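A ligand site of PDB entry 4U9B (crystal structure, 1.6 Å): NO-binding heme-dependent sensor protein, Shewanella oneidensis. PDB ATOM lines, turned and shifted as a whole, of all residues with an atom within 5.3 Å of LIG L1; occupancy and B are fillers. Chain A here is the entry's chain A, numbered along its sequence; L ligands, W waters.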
ATOM      1  N   MET A   1     -15.100   5.617  35.101  1.00  0.00           N
ATOM      2  CA  MET A   1     -15.309   4.654  33.997  1.00  0.00           C
ATOM      3  C   MET A   1     -15.772   3.315  34.577  1.00  0.00           C
ATOM      4  O   MET A   1     -15.030   2.663  35.302  1.00  0.00           O
ATOM      5  CB  MET A   1     -14.033   4.475  33.172  1.00  0.00           C
ATOM      6  CG  MET A   1     -14.223   3.759  31.831  1.00  0.00           C
ATOM      7  SD  MET A   1     -15.244   4.656  30.647  1.00  0.00           S
ATOM      8  CE  MET A   1     -14.247   6.104  30.352  1.00  0.00           C
ATOM      9  N   LYS A   2     -17.009   2.929  34.263  1.00  0.00           N
ATOM     10  CA  LYS A   2     -17.575   1.718  34.841  1.00  0.00           C
ATOM     11  C   LYS A   2     -16.932   0.469  34.242  1.00  0.00           C
ATOM     12  O   LYS A   2     -16.500   0.470  33.089  1.00  0.00           O
ATOM     13  CB  LYS A   2     -19.098   1.679  34.642  1.00  0.00           C
ATOM     14  CG  LYS A   2     -19.864   2.659  35.532  1.00  0.00           C
ATOM     15  CD  LYS A   2     -19.714   2.300  37.004  1.00  0.00           C
ATOM     16  CE  LYS A   2     -20.477   3.250  37.910  1.00  0.00           C
ATOM     17  NZ  LYS A   2     -20.126   3.020  39.350  1.00  0.00           N
ATOM     18  N   ILE A   4     -18.092  -2.210  33.139  1.00  0.00           N
ATOM     19  CA  ILE A   4     -18.735  -2.786  31.954  1.00  0.00           C
ATOM     20  C   ILE A   4     -17.987  -2.359  30.695  1.00  0.00           C
ATOM     21  O   ILE A   4     -17.808  -3.140  29.772  1.00  0.00           O
ATOM     22  CB  ILE A   4     -20.228  -2.387  31.842  1.00  0.00           C
ATOM     23  CG1 ILE A   4     -20.810  -2.905  30.521  1.00  0.00           C
ATOM     24  CG2 ILE A   4     -20.414  -0.887  31.928  1.00  0.00           C
ATOM     25  CD1 ILE A   4     -22.331  -2.975  30.504  1.00  0.00           C
ATOM     26  N   ILE A   5     -17.517  -1.110  30.675  1.00  0.00           N
ATOM     27  CA  ILE A   5     -16.779  -0.602  29.525  1.00  0.00           C
ATOM     28  C   ILE A   5     -15.491  -1.393  29.359  1.00  0.00           C
ATOM     29  O   ILE A   5     -15.138  -1.783  28.247  1.00  0.00           O
ATOM     30  CB  ILE A   5     -16.473   0.899  29.676  1.00  0.00           C
ATOM     31  CG1 ILE A   5     -17.757   1.690  29.937  1.00  0.00           C
ATOM     32  CG2 ILE A   5     -15.753   1.414  28.438  1.00  0.00           C
ATOM     33  CD1 ILE A   5     -18.811   1.572  28.850  1.00  0.00           C
ATOM     34  N   PHE A  74     -21.466  -0.972  21.155  1.00  0.00           N
ATOM     35  CA  PHE A  74     -22.915  -0.881  21.161  1.00  0.00           C
ATOM     36  C   PHE A  74     -23.544  -2.248  21.427  1.00  0.00           C
ATOM     37  O   PHE A  74     -24.440  -2.359  22.259  1.00  0.00           O
ATOM     38  CB  PHE A  74     -23.479  -0.336  19.847  1.00  0.00           C
ATOM     39  CG  PHE A  74     -24.967  -0.191  19.873  1.00  0.00           C
ATOM     40  CD1 PHE A  74     -25.548   0.954  20.371  1.00  0.00           C
ATOM     41  CD2 PHE A  74     -25.776  -1.234  19.459  1.00  0.00           C
ATOM     42  CE1 PHE A  74     -26.919   1.072  20.423  1.00  0.00           C
ATOM     43  CE2 PHE A  74     -27.147  -1.116  19.511  1.00  0.00           C
ATOM     44  CZ  PHE A  74     -27.722   0.039  19.990  1.00  0.00           C
ATOM     45  N   LEU A  77     -23.092  -3.315  25.011  1.00  0.00           N
ATOM     46  CA  LEU A  77     -24.049  -2.672  25.905  1.00  0.00           C
ATOM     47  C   LEU A  77     -25.453  -3.224  25.683  1.00  0.00           C
ATOM     48  O   LEU A  77     -26.191  -3.482  26.636  1.00  0.00           O
ATOM     49  CB  LEU A  77     -24.041  -1.158  25.709  1.00  0.00           C
ATOM     50  CG  LEU A  77     -22.772  -0.433  26.133  1.00  0.00           C
ATOM     51  CD1 LEU A  77     -22.776   0.996  25.624  1.00  0.00           C
ATOM     52  CD2 LEU A  77     -22.614  -0.456  27.646  1.00  0.00           C
ATOM     53  N   HIS A  81     -27.748  -5.004  28.476  1.00  0.00           N
ATOM     54  CA  HIS A  81     -28.908  -4.210  28.861  1.00  0.00           C
ATOM     55  C   HIS A  81     -29.982  -4.244  27.784  1.00  0.00           C
ATOM     56  O   HIS A  81     -30.394  -3.202  27.264  1.00  0.00           O
ATOM     57  CB  HIS A  81     -28.492  -2.766  29.149  1.00  0.00           C
ATOM     58  CG  HIS A  81     -27.523  -2.632  30.282  1.00  0.00           C
ATOM     59  ND1 HIS A  81     -27.854  -2.930  31.585  1.00  0.00           N
ATOM     60  CD2 HIS A  81     -26.229  -2.225  30.304  1.00  0.00           C
ATOM     61  CE1 HIS A  81     -26.806  -2.719  32.356  1.00  0.00           C
ATOM     62  NE2 HIS A  81     -25.805  -2.285  31.606  1.00  0.00           N
ATOM     63  N   VAL A  84     -33.185  -2.030  27.961  1.00  0.00           N
ATOM     64  CA  VAL A  84     -33.032  -0.619  27.627  1.00  0.00           C
ATOM     65  C   VAL A  84     -33.149  -0.399  26.126  1.00  0.00           C
ATOM     66  O   VAL A  84     -33.912   0.456  25.671  1.00  0.00           O
ATOM     67  CB  VAL A  84     -31.681  -0.069  28.127  1.00  0.00           C
ATOM     68  CG1 VAL A  84     -31.485   1.380  27.674  1.00  0.00           C
ATOM     69  CG2 VAL A  84     -31.602  -0.165  29.643  1.00  0.00           C
ATOM     70  N   VAL A  85     -32.396  -1.178  25.348  1.00  0.00           N
ATOM     71  CA  VAL A  85     -32.379  -1.020  23.901  1.00  0.00           C
ATOM     72  C   VAL A  85     -33.719  -1.405  23.290  1.00  0.00           C
ATOM     73  O   VAL A  85     -34.147  -0.798  22.308  1.00  0.00           O
ATOM     74  CB  VAL A  85     -31.254  -1.853  23.265  1.00  0.00           C
ATOM     75  CG1 VAL A  85     -31.232  -1.694  21.747  1.00  0.00           C
ATOM     76  CG2 VAL A  85     -29.903  -1.440  23.842  1.00  0.00           C
ATOM     77  N   LEU A  94     -33.825   5.817  19.132  1.00  0.00           N
ATOM     78  CA  LEU A  94     -32.736   5.524  20.062  1.00  0.00           C
ATOM     79  C   LEU A  94     -31.865   6.754  20.277  1.00  0.00           C
ATOM     80  O   LEU A  94     -31.614   7.158  21.420  1.00  0.00           O
ATOM     81  CB  LEU A  94     -31.870   4.360  19.549  1.00  0.00           C
ATOM     82  CG  LEU A  94     -30.814   3.803  20.514  1.00  0.00           C
ATOM     83  CD1 LEU A  94     -30.534   2.342  20.195  1.00  0.00           C
ATOM     84  CD2 LEU A  94     -29.512   4.599  20.467  1.00  0.00           C
ATOM     85  N   VAL A  95     -31.403   7.362  19.180  1.00  0.00           N
ATOM     86  CA  VAL A  95     -30.501   8.505  19.258  1.00  0.00           C
ATOM     87  C   VAL A  95     -31.162   9.682  19.981  1.00  0.00           C
ATOM     88  O   VAL A  95     -30.544  10.326  20.832  1.00  0.00           O
ATOM     89  CB  VAL A  95     -30.052   8.959  17.854  1.00  0.00           C
ATOM     90  CG1 VAL A  95     -29.150  10.184  17.946  1.00  0.00           C
ATOM     91  CG2 VAL A  95     -29.346   7.825  17.140  1.00  0.00           C
ATOM     92  N   ILE A  98     -31.200   9.133  23.784  1.00  0.00           N
ATOM     93  CA  ILE A  98     -29.974   9.020  24.585  1.00  0.00           C
ATOM     94  C   ILE A  98     -30.064   9.962  25.787  1.00  0.00           C
ATOM     95  O   ILE A  98     -29.740   9.567  26.917  1.00  0.00           O
ATOM     96  CB  ILE A  98     -28.713   9.364  23.756  1.00  0.00           C
ATOM     97  CG1 ILE A  98     -28.516   8.353  22.622  1.00  0.00           C
ATOM     98  CG2 ILE A  98     -27.467   9.386  24.650  1.00  0.00           C
ATOM     99  CD1 ILE A  98     -27.412   8.718  21.635  1.00  0.00           C
ATOM    100  N   ILE A 102     -31.850   6.741  27.808  1.00  0.00           N
ATOM    101  CA  ILE A 102     -30.613   6.038  28.149  1.00  0.00           C
ATOM    102  C   ILE A 102     -30.021   6.585  29.435  1.00  0.00           C
ATOM    103  O   ILE A 102     -29.668   5.815  30.330  1.00  0.00           O
ATOM    104  CB  ILE A 102     -29.558   6.163  27.030  1.00  0.00           C
ATOM    105  CG1 ILE A 102     -30.094   5.597  25.699  1.00  0.00           C
ATOM    106  CG2 ILE A 102     -28.262   5.443  27.437  1.00  0.00           C
ATOM    107  CD1 ILE A 102     -30.240   4.105  25.666  1.00  0.00           C
ATOM    108  N   VAL A 106     -29.487   4.242  32.772  1.00  0.00           N
ATOM    109  CA  VAL A 106     -28.142   3.999  33.259  1.00  0.00           C
ATOM    110  C   VAL A 106     -28.004   4.450  34.707  1.00  0.00           C
ATOM    111  O   VAL A 106     -27.357   3.787  35.512  1.00  0.00           O
ATOM    112  CB  VAL A 106     -27.077   4.714  32.393  1.00  0.00           C
ATOM    113  CG1 VAL A 106     -25.690   4.648  33.047  1.00  0.00           C
ATOM    114  CG2 VAL A 106     -27.021   4.103  31.004  1.00  0.00           C
ATOM    115  N   TYR A 110     -26.861   1.939  37.620  1.00  0.00           N
ATOM    116  CA  TYR A 110     -25.483   2.130  38.058  1.00  0.00           C
ATOM    117  C   TYR A 110     -25.389   3.193  39.148  1.00  0.00           C
ATOM    118  O   TYR A 110     -26.157   4.155  39.166  1.00  0.00           O
ATOM    119  CB  TYR A 110     -24.589   2.542  36.875  1.00  0.00           C
ATOM    120  CG  TYR A 110     -24.380   1.444  35.855  1.00  0.00           C
ATOM    121  CD1 TYR A 110     -25.284   1.257  34.818  1.00  0.00           C
ATOM    122  CD2 TYR A 110     -23.284   0.600  35.937  1.00  0.00           C
ATOM    123  CE1 TYR A 110     -25.093   0.248  33.889  1.00  0.00           C
ATOM    124  CE2 TYR A 110     -23.078  -0.409  35.007  1.00  0.00           C
ATOM    125  CZ  TYR A 110     -23.990  -0.581  33.986  1.00  0.00           C
ATOM    126  OH  TYR A 110     -23.800  -1.581  33.061  1.00  0.00           O
ATOM    127  N   GLU A 112     -23.722   6.299  40.498  1.00  0.00           N
ATOM    128  CA  GLU A 112     -22.932   7.464  40.117  1.00  0.00           C
ATOM    129  C   GLU A 112     -22.124   7.239  38.836  1.00  0.00           C
ATOM    130  O   GLU A 112     -20.895   7.318  38.841  1.00  0.00           O
ATOM    131  CB  GLU A 112     -21.992   7.859  41.257  1.00  0.00           C
ATOM    132  CG  GLU A 112     -22.715   8.396  42.475  1.00  0.00           C
ATOM    133  CD  GLU A 112     -21.767   8.925  43.545  1.00  0.00           C
ATOM    134  OE1 GLU A 112     -20.548   8.713  43.413  1.00  0.00           O
ATOM    135  OE2 GLU A 112     -22.260   9.559  44.500  1.00  0.00           O
ATOM    136  N   PRO A 113     -22.824   6.958  37.723  1.00  0.00           N
ATOM    137  CA  PRO A 113     -22.133   6.781  36.442  1.00  0.00           C
ATOM    138  C   PRO A 113     -21.596   8.114  35.932  1.00  0.00           C
ATOM    139  O   PRO A 113     -22.079   9.158  36.352  1.00  0.00           O
ATOM    140  CB  PRO A 113     -23.238   6.245  35.530  1.00  0.00           C
ATOM    141  CG  PRO A 113     -24.488   6.843  36.081  1.00  0.00           C
ATOM    142  CD  PRO A 113     -24.282   6.922  37.575  1.00  0.00           C
ATOM    143  N   SER A 114     -20.610   8.060  35.039  1.00  0.00           N
ATOM    144  CA  SER A 114     -20.066   9.254  34.401  1.00  0.00           C
ATOM    145  C   SER A 114     -20.434   9.247  32.921  1.00  0.00           C
ATOM    146  O   SER A 114     -19.729   8.679  32.090  1.00  0.00           O
ATOM    147  CB  SER A 114     -18.547   9.329  34.569  1.00  0.00           C
ATOM    148  OG  SER A 114     -18.211   9.497  35.939  1.00  0.00           O
ATOM    149  N   LEU A 115     -21.563   9.874  32.614  1.00  0.00           N
ATOM    150  CA  LEU A 115     -22.104   9.879  31.271  1.00  0.00           C
ATOM    151  C   LEU A 115     -21.756  11.175  30.554  1.00  0.00           C
ATOM    152  O   LEU A 115     -21.592  12.215  31.189  1.00  0.00           O
ATOM    153  CB  LEU A 115     -23.621   9.689  31.298  1.00  0.00           C
ATOM    154  CG  LEU A 115     -24.107   8.310  31.728  1.00  0.00           C
ATOM    155  CD1 LEU A 115     -25.605   8.338  31.998  1.00  0.00           C
ATOM    156  CD2 LEU A 115     -23.790   7.263  30.662  1.00  0.00           C
ATOM    157  N   PRO A 116     -21.631  11.112  29.214  1.00  0.00           N
ATOM    158  CA  PRO A 116     -21.400  12.347  28.470  1.00  0.00           C
ATOM    159  C   PRO A 116     -22.646  13.212  28.417  1.00  0.00           C
ATOM    160  O   PRO A 116     -23.746  12.711  28.642  1.00  0.00           O
ATOM    161  CB  PRO A 116     -21.020  11.845  27.083  1.00  0.00           C
ATOM    162  CG  PRO A 116     -21.755  10.559  26.957  1.00  0.00           C
ATOM    163  CD  PRO A 116     -21.702   9.941  28.331  1.00  0.00           C
ATOM    164  N   ILE A 118     -25.109  14.627  26.108  1.00  0.00           N
ATOM    165  CA  ILE A 118     -25.558  14.380  24.749  1.00  0.00           C
ATOM    166  C   ILE A 118     -26.975  14.937  24.572  1.00  0.00           C
ATOM    167  O   ILE A 118     -27.859  14.655  25.369  1.00  0.00           O
ATOM    168  CB  ILE A 118     -25.510  12.872  24.403  1.00  0.00           C
ATOM    169  CG1 ILE A 118     -24.040  12.451  24.209  1.00  0.00           C
ATOM    170  CG2 ILE A 118     -26.319  12.561  23.151  1.00  0.00           C
ATOM    171  CD1 ILE A 118     -23.829  10.978  23.906  1.00  0.00           C
ATOM    172  N   LEU A 130     -26.581  16.045  16.758  1.00  0.00           N
ATOM    173  CA  LEU A 130     -26.238  15.500  18.065  1.00  0.00           C
ATOM    174  C   LEU A 130     -25.071  16.260  18.678  1.00  0.00           C
ATOM    175  O   LEU A 130     -23.940  16.181  18.185  1.00  0.00           O
ATOM    176  CB  LEU A 130     -25.912  14.015  17.943  1.00  0.00           C
ATOM    177  CG  LEU A 130     -26.015  13.193  19.233  1.00  0.00           C
ATOM    178  CD1 LEU A 130     -27.443  13.185  19.778  1.00  0.00           C
ATOM    179  CD2 LEU A 130     -25.536  11.773  18.997  1.00  0.00           C
ATOM    180  N   TYR A 132     -22.342  16.756  21.531  1.00  0.00           N
ATOM    181  CA  TYR A 132     -21.599  15.940  22.484  1.00  0.00           C
ATOM    182  C   TYR A 132     -20.641  16.819  23.286  1.00  0.00           C
ATOM    183  O   TYR A 132     -19.929  17.655  22.724  1.00  0.00           O
ATOM    184  CB  TYR A 132     -20.824  14.836  21.763  1.00  0.00           C
ATOM    185  CG  TYR A 132     -19.868  14.075  22.654  1.00  0.00           C
ATOM    186  CD1 TYR A 132     -18.570  14.521  22.851  1.00  0.00           C
ATOM    187  CD2 TYR A 132     -20.265  12.914  23.290  1.00  0.00           C
ATOM    188  CE1 TYR A 132     -17.700  13.834  23.667  1.00  0.00           C
ATOM    189  CE2 TYR A 132     -19.394  12.212  24.114  1.00  0.00           C
ATOM    190  CZ  TYR A 132     -18.113  12.678  24.290  1.00  0.00           C
ATOM    191  OH  TYR A 132     -17.230  11.992  25.106  1.00  0.00           O
ATOM    192  N   SER A 134     -17.998  16.242  26.933  1.00  0.00           N
ATOM    193  CA  SER A 134     -17.545  15.384  28.029  1.00  0.00           C
ATOM    194  C   SER A 134     -16.083  15.640  28.390  1.00  0.00           C
ATOM    195  O   SER A 134     -15.253  15.852  27.501  1.00  0.00           O
ATOM    196  CB  SER A 134     -17.720  13.912  27.647  1.00  0.00           C
ATOM    197  OG  SER A 134     -17.172  13.071  28.650  1.00  0.00           O
ATOM    198  N   ARG A 136     -14.156  13.432  29.215  1.00  0.00           N
ATOM    199  CA  ARG A 136     -13.466  12.257  28.702  1.00  0.00           C
ATOM    200  C   ARG A 136     -13.033  12.446  27.245  1.00  0.00           C
ATOM    201  O   ARG A 136     -12.147  11.741  26.774  1.00  0.00           O
ATOM    202  CB  ARG A 136     -14.360  11.017  28.805  1.00  0.00           C
ATOM    203  CG  ARG A 136     -14.254  10.253  30.122  1.00  0.00           C
ATOM    204  CD  ARG A 136     -14.964  10.946  31.271  1.00  0.00           C
ATOM    205  NE  ARG A 136     -16.408  11.041  31.059  1.00  0.00           N
ATOM    206  CZ  ARG A 136     -17.242  11.704  31.859  1.00  0.00           C
ATOM    207  NH1 ARG A 136     -16.785  12.331  32.934  1.00  0.00           N
ATOM    208  NH2 ARG A 136     -18.534  11.740  31.583  1.00  0.00           N
ATOM    209  N   LEU A 138     -14.510  11.683  24.429  1.00  0.00           N
ATOM    210  CA  LEU A 138     -14.694  10.423  23.716  1.00  0.00           C
ATOM    211  C   LEU A 138     -15.705  10.531  22.583  1.00  0.00           C
ATOM    212  O   LEU A 138     -16.511   9.623  22.351  1.00  0.00           O
ATOM    213  CB  LEU A 138     -15.127   9.328  24.699  1.00  0.00           C
ATOM    214  CG  LEU A 138     -14.009   8.749  25.578  1.00  0.00           C
ATOM    215  CD1 LEU A 138     -14.604   7.979  26.741  1.00  0.00           C
ATOM    216  CD2 LEU A 138     -13.099   7.857  24.758  1.00  0.00           C
ATOM    217  N   CYS A 141     -15.750   7.710  20.230  1.00  0.00           N
ATOM    218  CA  CYS A 141     -16.450   6.554  20.766  1.00  0.00           C
ATOM    219  C   CYS A 141     -17.951   6.736  20.529  1.00  0.00           C
ATOM    220  O   CYS A 141     -18.657   5.779  20.203  1.00  0.00           O
ATOM    221  CB  CYS A 141     -16.136   6.366  22.252  1.00  0.00           C
ATOM    222  SG  CYS A 141     -16.842   4.865  23.001  1.00  0.00           S
ATOM    223  N   ALA A 142     -18.424   7.972  20.686  1.00  0.00           N
ATOM    224  CA  ALA A 142     -19.824   8.289  20.410  1.00  0.00           C
ATOM    225  C   ALA A 142     -20.156   8.031  18.950  1.00  0.00           C
ATOM    226  O   ALA A 142     -21.201   7.473  18.627  1.00  0.00           O
ATOM    227  CB  ALA A 142     -20.117   9.749  20.776  1.00  0.00           C
ATOM    228  N   LEU A 145     -20.328   4.327  18.433  1.00  0.00           N
ATOM    229  CA  LEU A 145     -21.568   3.792  19.012  1.00  0.00           C
ATOM    230  C   LEU A 145     -22.782   4.066  18.130  1.00  0.00           C
ATOM    231  O   LEU A 145     -23.690   3.250  18.043  1.00  0.00           O
ATOM    232  CB  LEU A 145     -21.793   4.389  20.408  1.00  0.00           C
ATOM    233  CG  LEU A 145     -20.985   3.723  21.521  1.00  0.00           C
ATOM    234  CD1 LEU A 145     -20.832   4.642  22.710  1.00  0.00           C
ATOM    235  CD2 LEU A 145     -21.656   2.419  21.930  1.00  0.00           C
ATOM    236  N   LEU A 146     -22.790   5.236  17.491  1.00  0.00           N
ATOM    237  CA  LEU A 146     -23.883   5.593  16.592  1.00  0.00           C
ATOM    238  C   LEU A 146     -23.907   4.657  15.385  1.00  0.00           C
ATOM    239  O   LEU A 146     -24.972   4.201  14.962  1.00  0.00           O
ATOM    240  CB  LEU A 146     -23.758   7.045  16.146  1.00  0.00           C
ATOM    241  CG  LEU A 146     -24.109   8.077  17.216  1.00  0.00           C
ATOM    242  CD1 LEU A 146     -23.533   9.436  16.864  1.00  0.00           C
ATOM    243  CD2 LEU A 146     -25.631   8.176  17.380  1.00  0.00           C
ATOM    244  N   ALA A 149     -25.193   1.381  16.588  1.00  0.00           N
ATOM    245  CA  ALA A 149     -26.648   1.438  16.735  1.00  0.00           C
ATOM    246  C   ALA A 149     -27.318   1.366  15.373  1.00  0.00           C
ATOM    247  O   ALA A 149     -28.383   0.778  15.225  1.00  0.00           O
ATOM    248  CB  ALA A 149     -27.052   2.702  17.472  1.00  0.00           C
HETATM  249  C1  LIG L   1     -20.714   5.763  28.339  1.00  0.00           C
HETATM  250  C2  LIG L   1     -22.439   7.550  24.189  1.00  0.00           C
HETATM  251  C3  LIG L   1     -25.754   4.046  24.007  1.00  0.00           C
HETATM  252  C4  LIG L   1     -24.785   3.042  28.647  1.00  0.00           C
HETATM  253  C5  LIG L   1     -20.785   6.421  27.134  1.00  0.00           C
HETATM  254  C6  LIG L   1     -19.713   7.139  26.473  1.00  0.00           C
HETATM  255  C7  LIG L   1     -20.209   7.629  25.331  1.00  0.00           C
HETATM  256  C8  LIG L   1     -21.587   7.245  25.225  1.00  0.00           C
HETATM  257  C9  LIG L   1     -19.444   8.458  24.277  1.00  0.00           C
HETATM  258  C10 LIG L   1     -18.266   7.315  27.001  1.00  0.00           C
HETATM  259  C11 LIG L   1     -18.240   8.236  28.217  1.00  0.00           C
HETATM  260  C12 LIG L   1     -18.114   9.703  27.856  1.00  0.00           C
HETATM  261  O1  LIG L   1     -18.057  10.549  28.791  1.00  0.00           O
HETATM  262  O2  LIG L   1     -18.082  10.049  26.645  1.00  0.00           O
HETATM  263  C13 LIG L   1     -23.453   6.732  23.740  1.00  0.00           C
HETATM  264  C14 LIG L   1     -24.090   6.807  22.446  1.00  0.00           C
HETATM  265  C15 LIG L   1     -25.020   5.840  22.391  1.00  0.00           C
HETATM  266  C16 LIG L   1     -24.970   5.123  23.647  1.00  0.00           C
HETATM  267  C17 LIG L   1     -23.715   7.877  21.393  1.00  0.00           C
HETATM  268  C18 LIG L   1     -25.995   5.439  21.258  1.00  0.00           C
HETATM  269  C19 LIG L   1     -25.816   5.783  19.980  1.00  0.00           C
HETATM  270  C20 LIG L   1     -25.786   3.461  25.254  1.00  0.00           C
HETATM  271  C21 LIG L   1     -26.652   2.368  25.660  1.00  0.00           C
HETATM  272  C22 LIG L   1     -26.417   2.083  26.942  1.00  0.00           C
HETATM  273  C23 LIG L   1     -25.360   2.987  27.403  1.00  0.00           C
HETATM  274  C24 LIG L   1     -27.681   1.689  24.730  1.00  0.00           C
HETATM  275  C25 LIG L   1     -27.153   0.966  27.718  1.00  0.00           C
HETATM  276  C26 LIG L   1     -27.106   0.835  29.047  1.00  0.00           C
HETATM  277  C27 LIG L   1     -23.556   3.597  28.955  1.00  0.00           C
HETATM  278  C28 LIG L   1     -22.796   3.284  30.136  1.00  0.00           C
HETATM  279  C29 LIG L   1     -21.529   4.134  30.039  1.00  0.00           C
HETATM  280  C30 LIG L   1     -21.645   4.879  28.809  1.00  0.00           C
HETATM  281  C31 LIG L   1     -23.168   2.299  31.267  1.00  0.00           C
HETATM  282  C32 LIG L   1     -20.360   4.189  31.041  1.00  0.00           C
HETATM  283  C33 LIG L   1     -20.615   5.259  32.090  1.00  0.00           C
HETATM  284  C34 LIG L   1     -19.439   5.293  33.042  1.00  0.00           C
HETATM  285  O3  LIG L   1     -18.354   4.795  32.653  1.00  0.00           O
HETATM  286  O4  LIG L   1     -19.595   5.803  34.187  1.00  0.00           O
HETATM  287  N1  LIG L   1     -21.922   6.493  26.339  1.00  0.00           N
HETATM  288  N2  LIG L   1     -24.000   5.694  24.445  1.00  0.00           N
HETATM  289  N3  LIG L   1     -25.013   3.809  26.354  1.00  0.00           N
HETATM  290  N4  LIG L   1     -22.853   4.536  28.199  1.00  0.00           N
HETATM  291 FE1  LIG L   1     -23.564   5.279  26.426  1.00  0.00          FE
HETATM  292  N1  LG2 L   2     -24.617   6.501  27.208  1.00  0.00           N
HETATM  293  O1  LG2 L   2     -24.798   7.850  26.706  1.00  0.00           O
HETATM  294  O   HOH W   1     -17.144   7.461  31.857  1.00  0.00           O
HETATM  295  O   HOH W   2     -17.707   5.608  36.183  1.00  0.00           O
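N of Ser 114 lies within hydrogen-bond range of O4 of LIG L1 (2.6 Å). OH of Tyr 132 sits at hydrogen-bond distance from O2 of LIG L1 (2.6 Å). An oxygen (O1) of LIG L1 is in hydrogen-bond range of the side-chain hydroxyl (OG) of Ser 134, at 2.7 Å. The backbone NH of Lys 2 is in hydrogen-bond range of an oxygen (O3) of LIG L1 (2.8 Å). The guanidinium group (NE) of Arg 136 is in salt-bridge range of an oxygen (O1) of LIG L1, at 2.8 Å.
An iron atom (FE1) of LIG L1 is bound by a nitrogen (N1) of LG2 L2, at 1.8 Å.
O of Ser 114 lies within hydrogen-bond range of NH2 of Arg 136. OH of Tyr 132 sits at hydrogen-bond distance from N of Leu 138, 2.8 Å away. OG of Ser 134 sits close to N of Arg 136, at 3.1 Å. O of Leu 115 is in hydrogen-bond range of NH2 of Arg 136, at 3.1 Å. NE2 of His 81 lies within hydrogen-bond range of OH of Tyr 110 (2.6 Å).
The side-chain sulfur (SD) of Met 1 lies close to an oxygen (O3) of LIG L1 (3.7 Å). Residues that only touch LIG L1: Ile 5, Leu 77, His 81, Val 85, Leu 94, Ile 98, Ile 102, Val 106, Tyr 110, Pro 113, Leu 115, Pro 116, Ile 118, Leu 138, Ala 142, Leu 145 and Leu 146. Hydrophobic or aromatic side chains that line LIG L1: Met 1, Ile 5, Leu 77, His 81, Val 85, Leu 94, Ile 98, Ile 102, Val 106, Tyr 110, Pro 113, Leu 115, Pro 116, Ile 118, Tyr 132, Leu 138, Ala 142, Leu 145 and Leu 146. Along chain A the residues within 4 Å of LIG L1 span positions 1 to 146. The nearest printed residue that does not touch LIG L1 is Ala 149 (4.2 Å).
Water W2 lies within hydrogen-bond range of an oxygen (O4) of LIG L1, the backbone NH (N) of Met 1 and the backbone NH (N) of Lys 2. Water W1 lies within hydrogen-bond range of the backbone carbonyl oxygen (O) of Ser 114 (2.9 Å), an oxygen (O3) of LIG L1 (3.0 Å) and the side-chain sulfur (SD) of Met 1 (3.6 Å).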
